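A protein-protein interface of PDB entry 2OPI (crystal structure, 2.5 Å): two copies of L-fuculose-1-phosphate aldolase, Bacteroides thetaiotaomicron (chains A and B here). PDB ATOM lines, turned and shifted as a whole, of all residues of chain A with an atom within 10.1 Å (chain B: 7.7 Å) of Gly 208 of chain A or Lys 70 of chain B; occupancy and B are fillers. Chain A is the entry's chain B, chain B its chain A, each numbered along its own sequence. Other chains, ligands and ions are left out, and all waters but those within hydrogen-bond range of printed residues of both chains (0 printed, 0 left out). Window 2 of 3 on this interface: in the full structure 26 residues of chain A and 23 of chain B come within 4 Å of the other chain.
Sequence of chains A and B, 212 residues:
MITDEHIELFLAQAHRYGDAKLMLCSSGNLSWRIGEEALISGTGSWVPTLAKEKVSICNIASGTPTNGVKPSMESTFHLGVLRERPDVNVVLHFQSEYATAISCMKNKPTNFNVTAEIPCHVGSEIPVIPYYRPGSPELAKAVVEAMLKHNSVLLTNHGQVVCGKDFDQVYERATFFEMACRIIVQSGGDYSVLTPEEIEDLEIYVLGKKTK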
ATOM      1  N   ASP A 201     -38.531   0.724  -0.572  1.00  0.00           N
ATOM      2  CA  ASP A 201     -37.999  -0.244   0.380  1.00  0.00           C
ATOM      3  C   ASP A 201     -37.034  -1.260  -0.266  1.00  0.00           C
ATOM      4  O   ASP A 201     -36.052  -1.684   0.355  1.00  0.00           O
ATOM      5  CB  ASP A 201     -39.182  -1.015   0.955  1.00  0.00           C
ATOM      6  CG  ASP A 201     -39.253  -0.948   2.460  1.00  0.00           C
ATOM      7  OD1 ASP A 201     -39.814   0.053   2.969  1.00  0.00           O
ATOM      8  OD2 ASP A 201     -38.780  -1.908   3.127  1.00  0.00           O
ATOM      9  N   LEU A 202     -37.324  -1.643  -1.509  1.00  0.00           N
ATOM     10  CA  LEU A 202     -36.528  -2.623  -2.238  1.00  0.00           C
ATOM     11  C   LEU A 202     -35.054  -2.240  -2.462  1.00  0.00           C
ATOM     12  O   LEU A 202     -34.224  -3.118  -2.684  1.00  0.00           O
ATOM     13  CB  LEU A 202     -37.211  -2.989  -3.560  1.00  0.00           C
ATOM     14  CG  LEU A 202     -38.542  -3.748  -3.485  1.00  0.00           C
ATOM     15  CD1 LEU A 202     -39.112  -4.006  -4.870  1.00  0.00           C
ATOM     16  CD2 LEU A 202     -38.396  -5.055  -2.750  1.00  0.00           C
ATOM     17  N   GLU A 203     -34.742  -0.942  -2.381  1.00  0.00           N
ATOM     18  CA  GLU A 203     -33.369  -0.420  -2.511  1.00  0.00           C
ATOM     19  C   GLU A 203     -32.412  -1.139  -1.556  1.00  0.00           C
ATOM     20  O   GLU A 203     -31.286  -1.468  -1.925  1.00  0.00           O
ATOM     21  CB  GLU A 203     -33.337   1.096  -2.243  1.00  0.00           C
ATOM     22  CG  GLU A 203     -33.548   1.470  -0.747  1.00  0.00           C
ATOM     23  CD  GLU A 203     -33.711   2.971  -0.460  1.00  0.00           C
ATOM     24  OE1 GLU A 203     -33.927   3.770  -1.410  1.00  0.00           O
ATOM     25  OE2 GLU A 203     -33.630   3.353   0.737  1.00  0.00           O
ATOM     26  N   ILE A 204     -32.889  -1.380  -0.333  1.00  0.00           N
ATOM     27  CA  ILE A 204     -32.157  -2.087   0.725  1.00  0.00           C
ATOM     28  C   ILE A 204     -31.924  -3.549   0.365  1.00  0.00           C
ATOM     29  O   ILE A 204     -30.851  -4.103   0.625  1.00  0.00           O
ATOM     30  CB  ILE A 204     -32.936  -2.028   2.072  1.00  0.00           C
ATOM     31  CG1 ILE A 204     -33.222  -0.579   2.465  1.00  0.00           C
ATOM     32  CG2 ILE A 204     -32.172  -2.747   3.184  1.00  0.00           C
ATOM     33  CD1 ILE A 204     -31.980   0.306   2.435  1.00  0.00           C
ATOM     34  N   TYR A 205     -32.946  -4.163  -0.218  1.00  0.00           N
ATOM     35  CA  TYR A 205     -32.863  -5.523  -0.690  1.00  0.00           C
ATOM     36  C   TYR A 205     -31.873  -5.629  -1.858  1.00  0.00           C
ATOM     37  O   TYR A 205     -31.034  -6.529  -1.876  1.00  0.00           O
ATOM     38  CB  TYR A 205     -34.254  -6.016  -1.079  1.00  0.00           C
ATOM     39  CG  TYR A 205     -34.286  -7.399  -1.663  1.00  0.00           C
ATOM     40  CD1 TYR A 205     -33.857  -8.505  -0.920  1.00  0.00           C
ATOM     41  CD2 TYR A 205     -34.765  -7.614  -2.956  1.00  0.00           C
ATOM     42  CE1 TYR A 205     -33.893  -9.794  -1.455  1.00  0.00           C
ATOM     43  CE2 TYR A 205     -34.810  -8.896  -3.507  1.00  0.00           C
ATOM     44  CZ  TYR A 205     -34.372  -9.980  -2.750  1.00  0.00           C
ATOM     45  OH  TYR A 205     -34.415 -11.244  -3.287  1.00  0.00           O
ATOM     46  N   VAL A 206     -31.952  -4.695  -2.804  1.00  0.00           N
ATOM     47  CA  VAL A 206     -31.042  -4.656  -3.957  1.00  0.00           C
ATOM     48  C   VAL A 206     -29.591  -4.441  -3.515  1.00  0.00           C
ATOM     49  O   VAL A 206     -28.682  -5.115  -4.008  1.00  0.00           O
ATOM     50  CB  VAL A 206     -31.467  -3.581  -4.993  1.00  0.00           C
ATOM     51  CG1 VAL A 206     -30.446  -3.452  -6.117  1.00  0.00           C
ATOM     52  CG2 VAL A 206     -32.826  -3.918  -5.576  1.00  0.00           C
ATOM     53  N   LEU A 207     -29.382  -3.516  -2.582  1.00  0.00           N
ATOM     54  CA  LEU A 207     -28.080  -3.346  -1.941  1.00  0.00           C
ATOM     55  C   LEU A 207     -27.499  -4.655  -1.410  1.00  0.00           C
ATOM     56  O   LEU A 207     -26.420  -5.078  -1.839  1.00  0.00           O
ATOM     57  CB  LEU A 207     -28.152  -2.317  -0.808  1.00  0.00           C
ATOM     58  CG  LEU A 207     -27.521  -0.959  -1.136  1.00  0.00           C
ATOM     59  CD1 LEU A 207     -27.944   0.116  -0.124  1.00  0.00           C
ATOM     60  CD2 LEU A 207     -25.987  -1.076  -1.226  1.00  0.00           C
ATOM     61  N   GLY A 208     -28.226  -5.295  -0.494  1.00  0.00           N
ATOM     62  CA  GLY A 208     -27.816  -6.571   0.073  1.00  0.00           C
ATOM     63  C   GLY A 208     -27.390  -7.599  -0.961  1.00  0.00           C
ATOM     64  O   GLY A 208     -26.476  -8.386  -0.713  1.00  0.00           O
ATOM     65  N   LYS A 209     -28.054  -7.601  -2.118  1.00  0.00           N
ATOM     66  CA  LYS A 209     -27.705  -8.520  -3.202  1.00  0.00           C
ATOM     67  C   LYS A 209     -26.363  -8.125  -3.812  1.00  0.00           C
ATOM     68  O   LYS A 209     -25.733  -8.913  -4.511  1.00  0.00           O
ATOM     69  CB  LYS A 209     -28.789  -8.537  -4.283  1.00  0.00           C
ATOM     70  CG  LYS A 209     -29.978  -9.432  -3.984  1.00  0.00           C
ATOM     71  CD  LYS A 209     -30.822  -9.619  -5.238  1.00  0.00           C
ATOM     72  CE  LYS A 209     -31.590 -10.946  -5.233  1.00  0.00           C
ATOM     73  NZ  LYS A 209     -31.788 -11.504  -6.618  1.00  0.00           N
ATOM     74  N   ILE B  40     -27.128 -23.220   1.283  1.00  0.00           N
ATOM     75  CA  ILE B  40     -28.111 -22.229   0.856  1.00  0.00           C
ATOM     76  C   ILE B  40     -27.625 -21.653  -0.462  1.00  0.00           C
ATOM     77  O   ILE B  40     -26.437 -21.378  -0.627  1.00  0.00           O
ATOM     78  CB  ILE B  40     -28.292 -21.086   1.892  1.00  0.00           C
ATOM     79  CG1 ILE B  40     -28.114 -21.626   3.314  1.00  0.00           C
ATOM     80  CG2 ILE B  40     -29.666 -20.437   1.737  1.00  0.00           C
ATOM     81  CD1 ILE B  40     -28.313 -20.617   4.427  1.00  0.00           C
ATOM     82  N   SER B  41     -28.541 -21.497  -1.409  1.00  0.00           N
ATOM     83  CA  SER B  41     -28.243 -20.792  -2.645  1.00  0.00           C
ATOM     84  C   SER B  41     -27.756 -19.383  -2.318  1.00  0.00           C
ATOM     85  O   SER B  41     -28.287 -18.722  -1.418  1.00  0.00           O
ATOM     86  CB  SER B  41     -29.493 -20.717  -3.509  1.00  0.00           C
ATOM     87  OG  SER B  41     -30.486 -19.933  -2.875  1.00  0.00           O
ATOM     88  N   GLY B  42     -26.747 -18.935  -3.055  1.00  0.00           N
ATOM     89  CA  GLY B  42     -26.100 -17.653  -2.793  1.00  0.00           C
ATOM     90  C   GLY B  42     -26.980 -16.503  -3.222  1.00  0.00           C
ATOM     91  O   GLY B  42     -27.784 -16.643  -4.148  1.00  0.00           O
ATOM     92  N   THR B  43     -26.828 -15.360  -2.560  1.00  0.00           N
ATOM     93  CA  THR B  43     -27.642 -14.197  -2.880  1.00  0.00           C
ATOM     94  C   THR B  43     -27.439 -13.805  -4.335  1.00  0.00           C
ATOM     95  O   THR B  43     -26.313 -13.802  -4.832  1.00  0.00           O
ATOM     96  CB  THR B  43     -27.371 -13.002  -1.917  1.00  0.00           C
ATOM     97  OG1 THR B  43     -28.427 -12.038  -2.038  1.00  0.00           O
ATOM     98  CG2 THR B  43     -26.016 -12.338  -2.194  1.00  0.00           C
ATOM     99  N   GLY B  44     -28.533 -13.513  -5.027  1.00  0.00           N
ATOM    100  CA  GLY B  44     -28.458 -13.087  -6.416  1.00  0.00           C
ATOM    101  C   GLY B  44     -28.280 -14.202  -7.431  1.00  0.00           C
ATOM    102  O   GLY B  44     -28.489 -13.994  -8.620  1.00  0.00           O
ATOM    103  N   SER B  45     -27.904 -15.390  -6.977  1.00  0.00           N
ATOM    104  CA  SER B  45     -27.697 -16.512  -7.890  1.00  0.00           C
ATOM    105  C   SER B  45     -28.997 -16.901  -8.603  1.00  0.00           C
ATOM    106  O   SER B  45     -30.096 -16.673  -8.081  1.00  0.00           O
ATOM    107  CB  SER B  45     -27.177 -17.714  -7.121  1.00  0.00           C
ATOM    108  OG  SER B  45     -28.215 -18.249  -6.314  1.00  0.00           O
ATOM    109  N   GLU B  53     -20.055 -22.152  -7.700  1.00  0.00           N
ATOM    110  CA  GLU B  53     -19.408 -21.003  -7.078  1.00  0.00           C
ATOM    111  C   GLU B  53     -20.361 -20.160  -6.214  1.00  0.00           C
ATOM    112  O   GLU B  53     -19.903 -19.332  -5.416  1.00  0.00           O
ATOM    113  CB  GLU B  53     -18.762 -20.116  -8.160  1.00  0.00           C
ATOM    114  CG  GLU B  53     -17.406 -20.601  -8.683  1.00  0.00           C
ATOM    115  CD  GLU B  53     -17.462 -21.948  -9.411  1.00  0.00           C
ATOM    116  OE1 GLU B  53     -18.559 -22.344  -9.888  1.00  0.00           O
ATOM    117  OE2 GLU B  53     -16.395 -22.609  -9.506  1.00  0.00           O
ATOM    118  N   LYS B  54     -21.673 -20.355  -6.380  1.00  0.00           N
ATOM    119  CA  LYS B  54     -22.668 -19.528  -5.677  1.00  0.00           C
ATOM    120  C   LYS B  54     -23.559 -20.350  -4.740  1.00  0.00           C
ATOM    121  O   LYS B  54     -24.765 -20.121  -4.644  1.00  0.00           O
ATOM    122  CB  LYS B  54     -23.502 -18.691  -6.662  1.00  0.00           C
ATOM    123  CG  LYS B  54     -22.680 -18.051  -7.776  1.00  0.00           C
ATOM    124  CD  LYS B  54     -23.315 -16.784  -8.318  1.00  0.00           C
ATOM    125  CE  LYS B  54     -22.534 -15.537  -7.892  1.00  0.00           C
ATOM    126  NZ  LYS B  54     -23.160 -14.297  -8.455  1.00  0.00           N
ATOM    127  N   VAL B  55     -22.937 -21.312  -4.061  1.00  0.00           N
ATOM    128  CA  VAL B  55     -23.580 -22.083  -3.008  1.00  0.00           C
ATOM    129  C   VAL B  55     -22.909 -21.784  -1.673  1.00  0.00           C
ATOM    130  O   VAL B  55     -21.701 -21.966  -1.525  1.00  0.00           O
ATOM    131  CB  VAL B  55     -23.491 -23.595  -3.269  1.00  0.00           C
ATOM    132  CG1 VAL B  55     -24.040 -24.381  -2.058  1.00  0.00           C
ATOM    133  CG2 VAL B  55     -24.240 -23.960  -4.544  1.00  0.00           C
ATOM    134  N   SER B  56     -23.711 -21.337  -0.711  1.00  0.00           N
ATOM    135  CA  SER B  56     -23.248 -20.971   0.613  1.00  0.00           C
ATOM    136  C   SER B  56     -23.337 -22.144   1.576  1.00  0.00           C
ATOM    137  O   SER B  56     -24.325 -22.865   1.600  1.00  0.00           O
ATOM    138  CB  SER B  56     -24.106 -19.825   1.132  1.00  0.00           C
ATOM    139  OG  SER B  56     -23.516 -19.194   2.246  1.00  0.00           O
ATOM    140  N   ILE B  57     -22.282 -22.334   2.358  1.00  0.00           N
ATOM    141  CA  ILE B  57     -22.311 -23.227   3.503  1.00  0.00           C
ATOM    142  C   ILE B  57     -22.444 -22.337   4.737  1.00  0.00           C
ATOM    143  O   ILE B  57     -21.648 -21.422   4.940  1.00  0.00           O
ATOM    144  CB  ILE B  57     -21.029 -24.063   3.596  1.00  0.00           C
ATOM    145  CG1 ILE B  57     -20.860 -24.914   2.327  1.00  0.00           C
ATOM    146  CG2 ILE B  57     -21.034 -24.929   4.859  1.00  0.00           C
ATOM    147  CD1 ILE B  57     -19.399 -25.345   2.022  1.00  0.00           C
ATOM    148  N   CYS B  58     -23.469 -22.590   5.538  1.00  0.00           N
ATOM    149  CA  CYS B  58     -23.783 -21.755   6.693  1.00  0.00           C
ATOM    150  C   CYS B  58     -23.946 -22.570   7.961  1.00  0.00           C
ATOM    151  O   CYS B  58     -24.561 -23.638   7.950  1.00  0.00           O
ATOM    152  CB  CYS B  58     -25.067 -20.967   6.440  1.00  0.00           C
ATOM    153  SG  CYS B  58     -24.804 -19.527   5.384  1.00  0.00           S
ATOM    154  N   PRO B  65     -21.863 -17.690   6.971  1.00  0.00           N
ATOM    155  CA  PRO B  65     -21.201 -18.508   5.943  1.00  0.00           C
ATOM    156  C   PRO B  65     -19.782 -18.888   6.334  1.00  0.00           C
ATOM    157  O   PRO B  65     -19.118 -18.120   7.017  1.00  0.00           O
ATOM    158  CB  PRO B  65     -21.172 -17.584   4.711  1.00  0.00           C
ATOM    159  CG  PRO B  65     -21.325 -16.199   5.253  1.00  0.00           C
ATOM    160  CD  PRO B  65     -22.196 -16.340   6.470  1.00  0.00           C
ATOM    161  N   ASN B  67     -17.702 -20.515   3.708  1.00  0.00           N
ATOM    162  CA  ASN B  67     -16.983 -20.751   2.449  1.00  0.00           C
ATOM    163  C   ASN B  67     -16.770 -19.518   1.554  1.00  0.00           C
ATOM    164  O   ASN B  67     -16.431 -19.660   0.385  1.00  0.00           O
ATOM    165  CB  ASN B  67     -17.644 -21.895   1.656  1.00  0.00           C
ATOM    166  CG  ASN B  67     -19.058 -21.558   1.168  1.00  0.00           C
ATOM    167  OD1 ASN B  67     -19.622 -22.297   0.364  1.00  0.00           O
ATOM    168  ND2 ASN B  67     -19.635 -20.447   1.650  1.00  0.00           N
ATOM    169  N   GLY B  68     -16.971 -18.321   2.099  1.00  0.00           N
ATOM    170  CA  GLY B  68     -16.791 -17.096   1.327  1.00  0.00           C
ATOM    171  C   GLY B  68     -17.933 -16.773   0.374  1.00  0.00           C
ATOM    172  O   GLY B  68     -17.813 -15.862  -0.454  1.00  0.00           O
ATOM    173  N   VAL B  69     -19.045 -17.499   0.482  1.00  0.00           N
ATOM    174  CA  VAL B  69     -20.211 -17.236  -0.369  1.00  0.00           C
ATOM    175  C   VAL B  69     -21.384 -16.632   0.426  1.00  0.00           C
ATOM    176  O   VAL B  69     -21.922 -17.248   1.363  1.00  0.00           O
ATOM    177  CB  VAL B  69     -20.676 -18.506  -1.158  1.00  0.00           C
ATOM    178  CG1 VAL B  69     -21.854 -18.175  -2.045  1.00  0.00           C
ATOM    179  CG2 VAL B  69     -19.509 -19.107  -1.980  1.00  0.00           C
ATOM    180  N   LYS B  70     -21.761 -15.415   0.043  1.00  0.00           N
ATOM    181  CA  LYS B  70     -22.838 -14.705   0.695  1.00  0.00           C
ATOM    182  C   LYS B  70     -24.138 -15.447   0.410  1.00  0.00           C
ATOM    183  O   LYS B  70     -24.514 -15.650  -0.754  1.00  0.00           O
ATOM    184  CB  LYS B  70     -22.900 -13.272   0.190  1.00  0.00           C
ATOM    185  CG  LYS B  70     -23.614 -12.277   1.104  1.00  0.00           C
ATOM    186  CD  LYS B  70     -23.557 -10.898   0.461  1.00  0.00           C
ATOM    187  CE  LYS B  70     -23.903  -9.788   1.426  1.00  0.00           C
ATOM    188  NZ  LYS B  70     -25.342  -9.748   1.784  1.00  0.00           N
ATOM    189  N   PRO B  71     -24.820 -15.881   1.482  1.00  0.00           N
ATOM    190  CA  PRO B  71     -26.048 -16.657   1.341  1.00  0.00           C
ATOM    191  C   PRO B  71     -27.199 -15.756   0.911  1.00  0.00           C
ATOM    192  O   PRO B  71     -27.128 -14.544   1.091  1.00  0.00           O
ATOM    193  CB  PRO B  71     -26.287 -17.176   2.757  1.00  0.00           C
ATOM    194  CG  PRO B  71     -25.666 -16.145   3.632  1.00  0.00           C
ATOM    195  CD  PRO B  71     -24.471 -15.634   2.896  1.00  0.00           C
ATOM    196  N   SER B  72     -28.233 -16.357   0.332  1.00  0.00           N
ATOM    197  CA  SER B  72     -29.515 -15.713   0.095  1.00  0.00           C
ATOM    198  C   SER B  72     -29.910 -14.769   1.245  1.00  0.00           C
ATOM    199  O   SER B  72     -29.726 -15.105   2.414  1.00  0.00           O
ATOM    200  CB  SER B  72     -30.570 -16.819  -0.061  1.00  0.00           C
ATOM    201  OG  SER B  72     -31.898 -16.349   0.070  1.00  0.00           O
ATOM    202  N   MET B  73     -30.425 -13.584   0.917  1.00  0.00           N
ATOM    203  CA  MET B  73     -31.229 -12.819   1.877  1.00  0.00           C
ATOM    204  C   MET B  73     -32.393 -13.763   2.103  1.00  0.00           C
ATOM    205  O   MET B  73     -32.674 -14.608   1.249  1.00  0.00           O
ATOM    206  CB  MET B  73     -31.743 -11.515   1.273  1.00  0.00           C
ATOM    207  CG  MET B  73     -30.746 -10.778   0.389  1.00  0.00           C
ATOM    208  SD  MET B  73     -29.455  -9.723   1.425  1.00  0.00           S
ATOM    209  CE  MET B  73     -30.678  -8.248   1.936  1.00  0.00           C
ATOM    210  N   SER B  75     -32.173 -16.079   4.104  1.00  0.00           N
ATOM    211  CA  SER B  75     -31.503 -17.124   4.870  1.00  0.00           C
ATOM    212  C   SER B  75     -32.053 -17.088   6.285  1.00  0.00           C
ATOM    213  O   SER B  75     -32.016 -18.075   7.017  1.00  0.00           O
ATOM    214  CB  SER B  75     -30.011 -16.841   4.937  1.00  0.00           C
ATOM    215  OG  SER B  75     -29.774 -15.656   5.687  1.00  0.00           O
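NZ of Lys 70 of chain B lies within hydrogen-bond range of O of Gly 208 of chain A (3.1 Å).
N of Thr 43 of chain B is in hydrogen-bond range of O of Lys 70 of chain B, at 2.9 Å.
CG of Met 73 of chain B touches CE1 of Tyr 205 of chain A, at 3.8 Å. CA of Gly 208 of chain A touches SD of Met 73 of chain B, at 3.8 Å. Lys 209 of chain A touches Thr 43 of chain B (CG to OG1, 3.6 Å). Lys 209 of chain A touches Gly 44 of chain B.
Of chain B, only Lys 70 and Met 73 come within 4 Å of Gly 208 of chain A. Printed residues of chain B within 4 Å of Lys 209 of chain A: Thr 43 (3.6 Å) and Gly 44 (3.7 Å). Ile 40 of chain B touches none of the printed residues of chain A. No residue of chain A comes within 4 Å of Gly 42 of chain B. Thr 43 of chain B touches just one residue of chain A: Lys 209. Printed residues of chain A within 4 Å of Gly 44 of chain B: Lys 209. No residue of chain A comes within 4 Å of Gly 68 of chain B. Of chain A, only Gly 208 comes within 4 Å of Lys 70 of chain B. Printed residues of chain A within 4 Å of Met 73 of chain B: Tyr 205 (3.8 Å) and Gly 208 (3.8 Å). The nearest residue of chain A that does not touch Lys 70 of chain B is Lys 209 of chain A (5.2 Å). The nearest printed residue of chain A that does not touch Gly 44 of chain B is Tyr 205 of chain A (6.5 Å).
Of the 9 printed residues of chain A, 3 touch a printed residue of chain B. Of the 21 printed residues of chain B, 4 touch a printed residue of chain A. Among the printed residues, 5 pairs touch across the chains. Among the printed residues, no Asp or Glu carboxylate lies within 4 Å of a Lys or Arg side-chain nitrogen of the other chain.
No position is printed for both chains. Of the 5 pairs that touch across the chains among the printed residues, none has its exchanged pair printed and touching as well.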
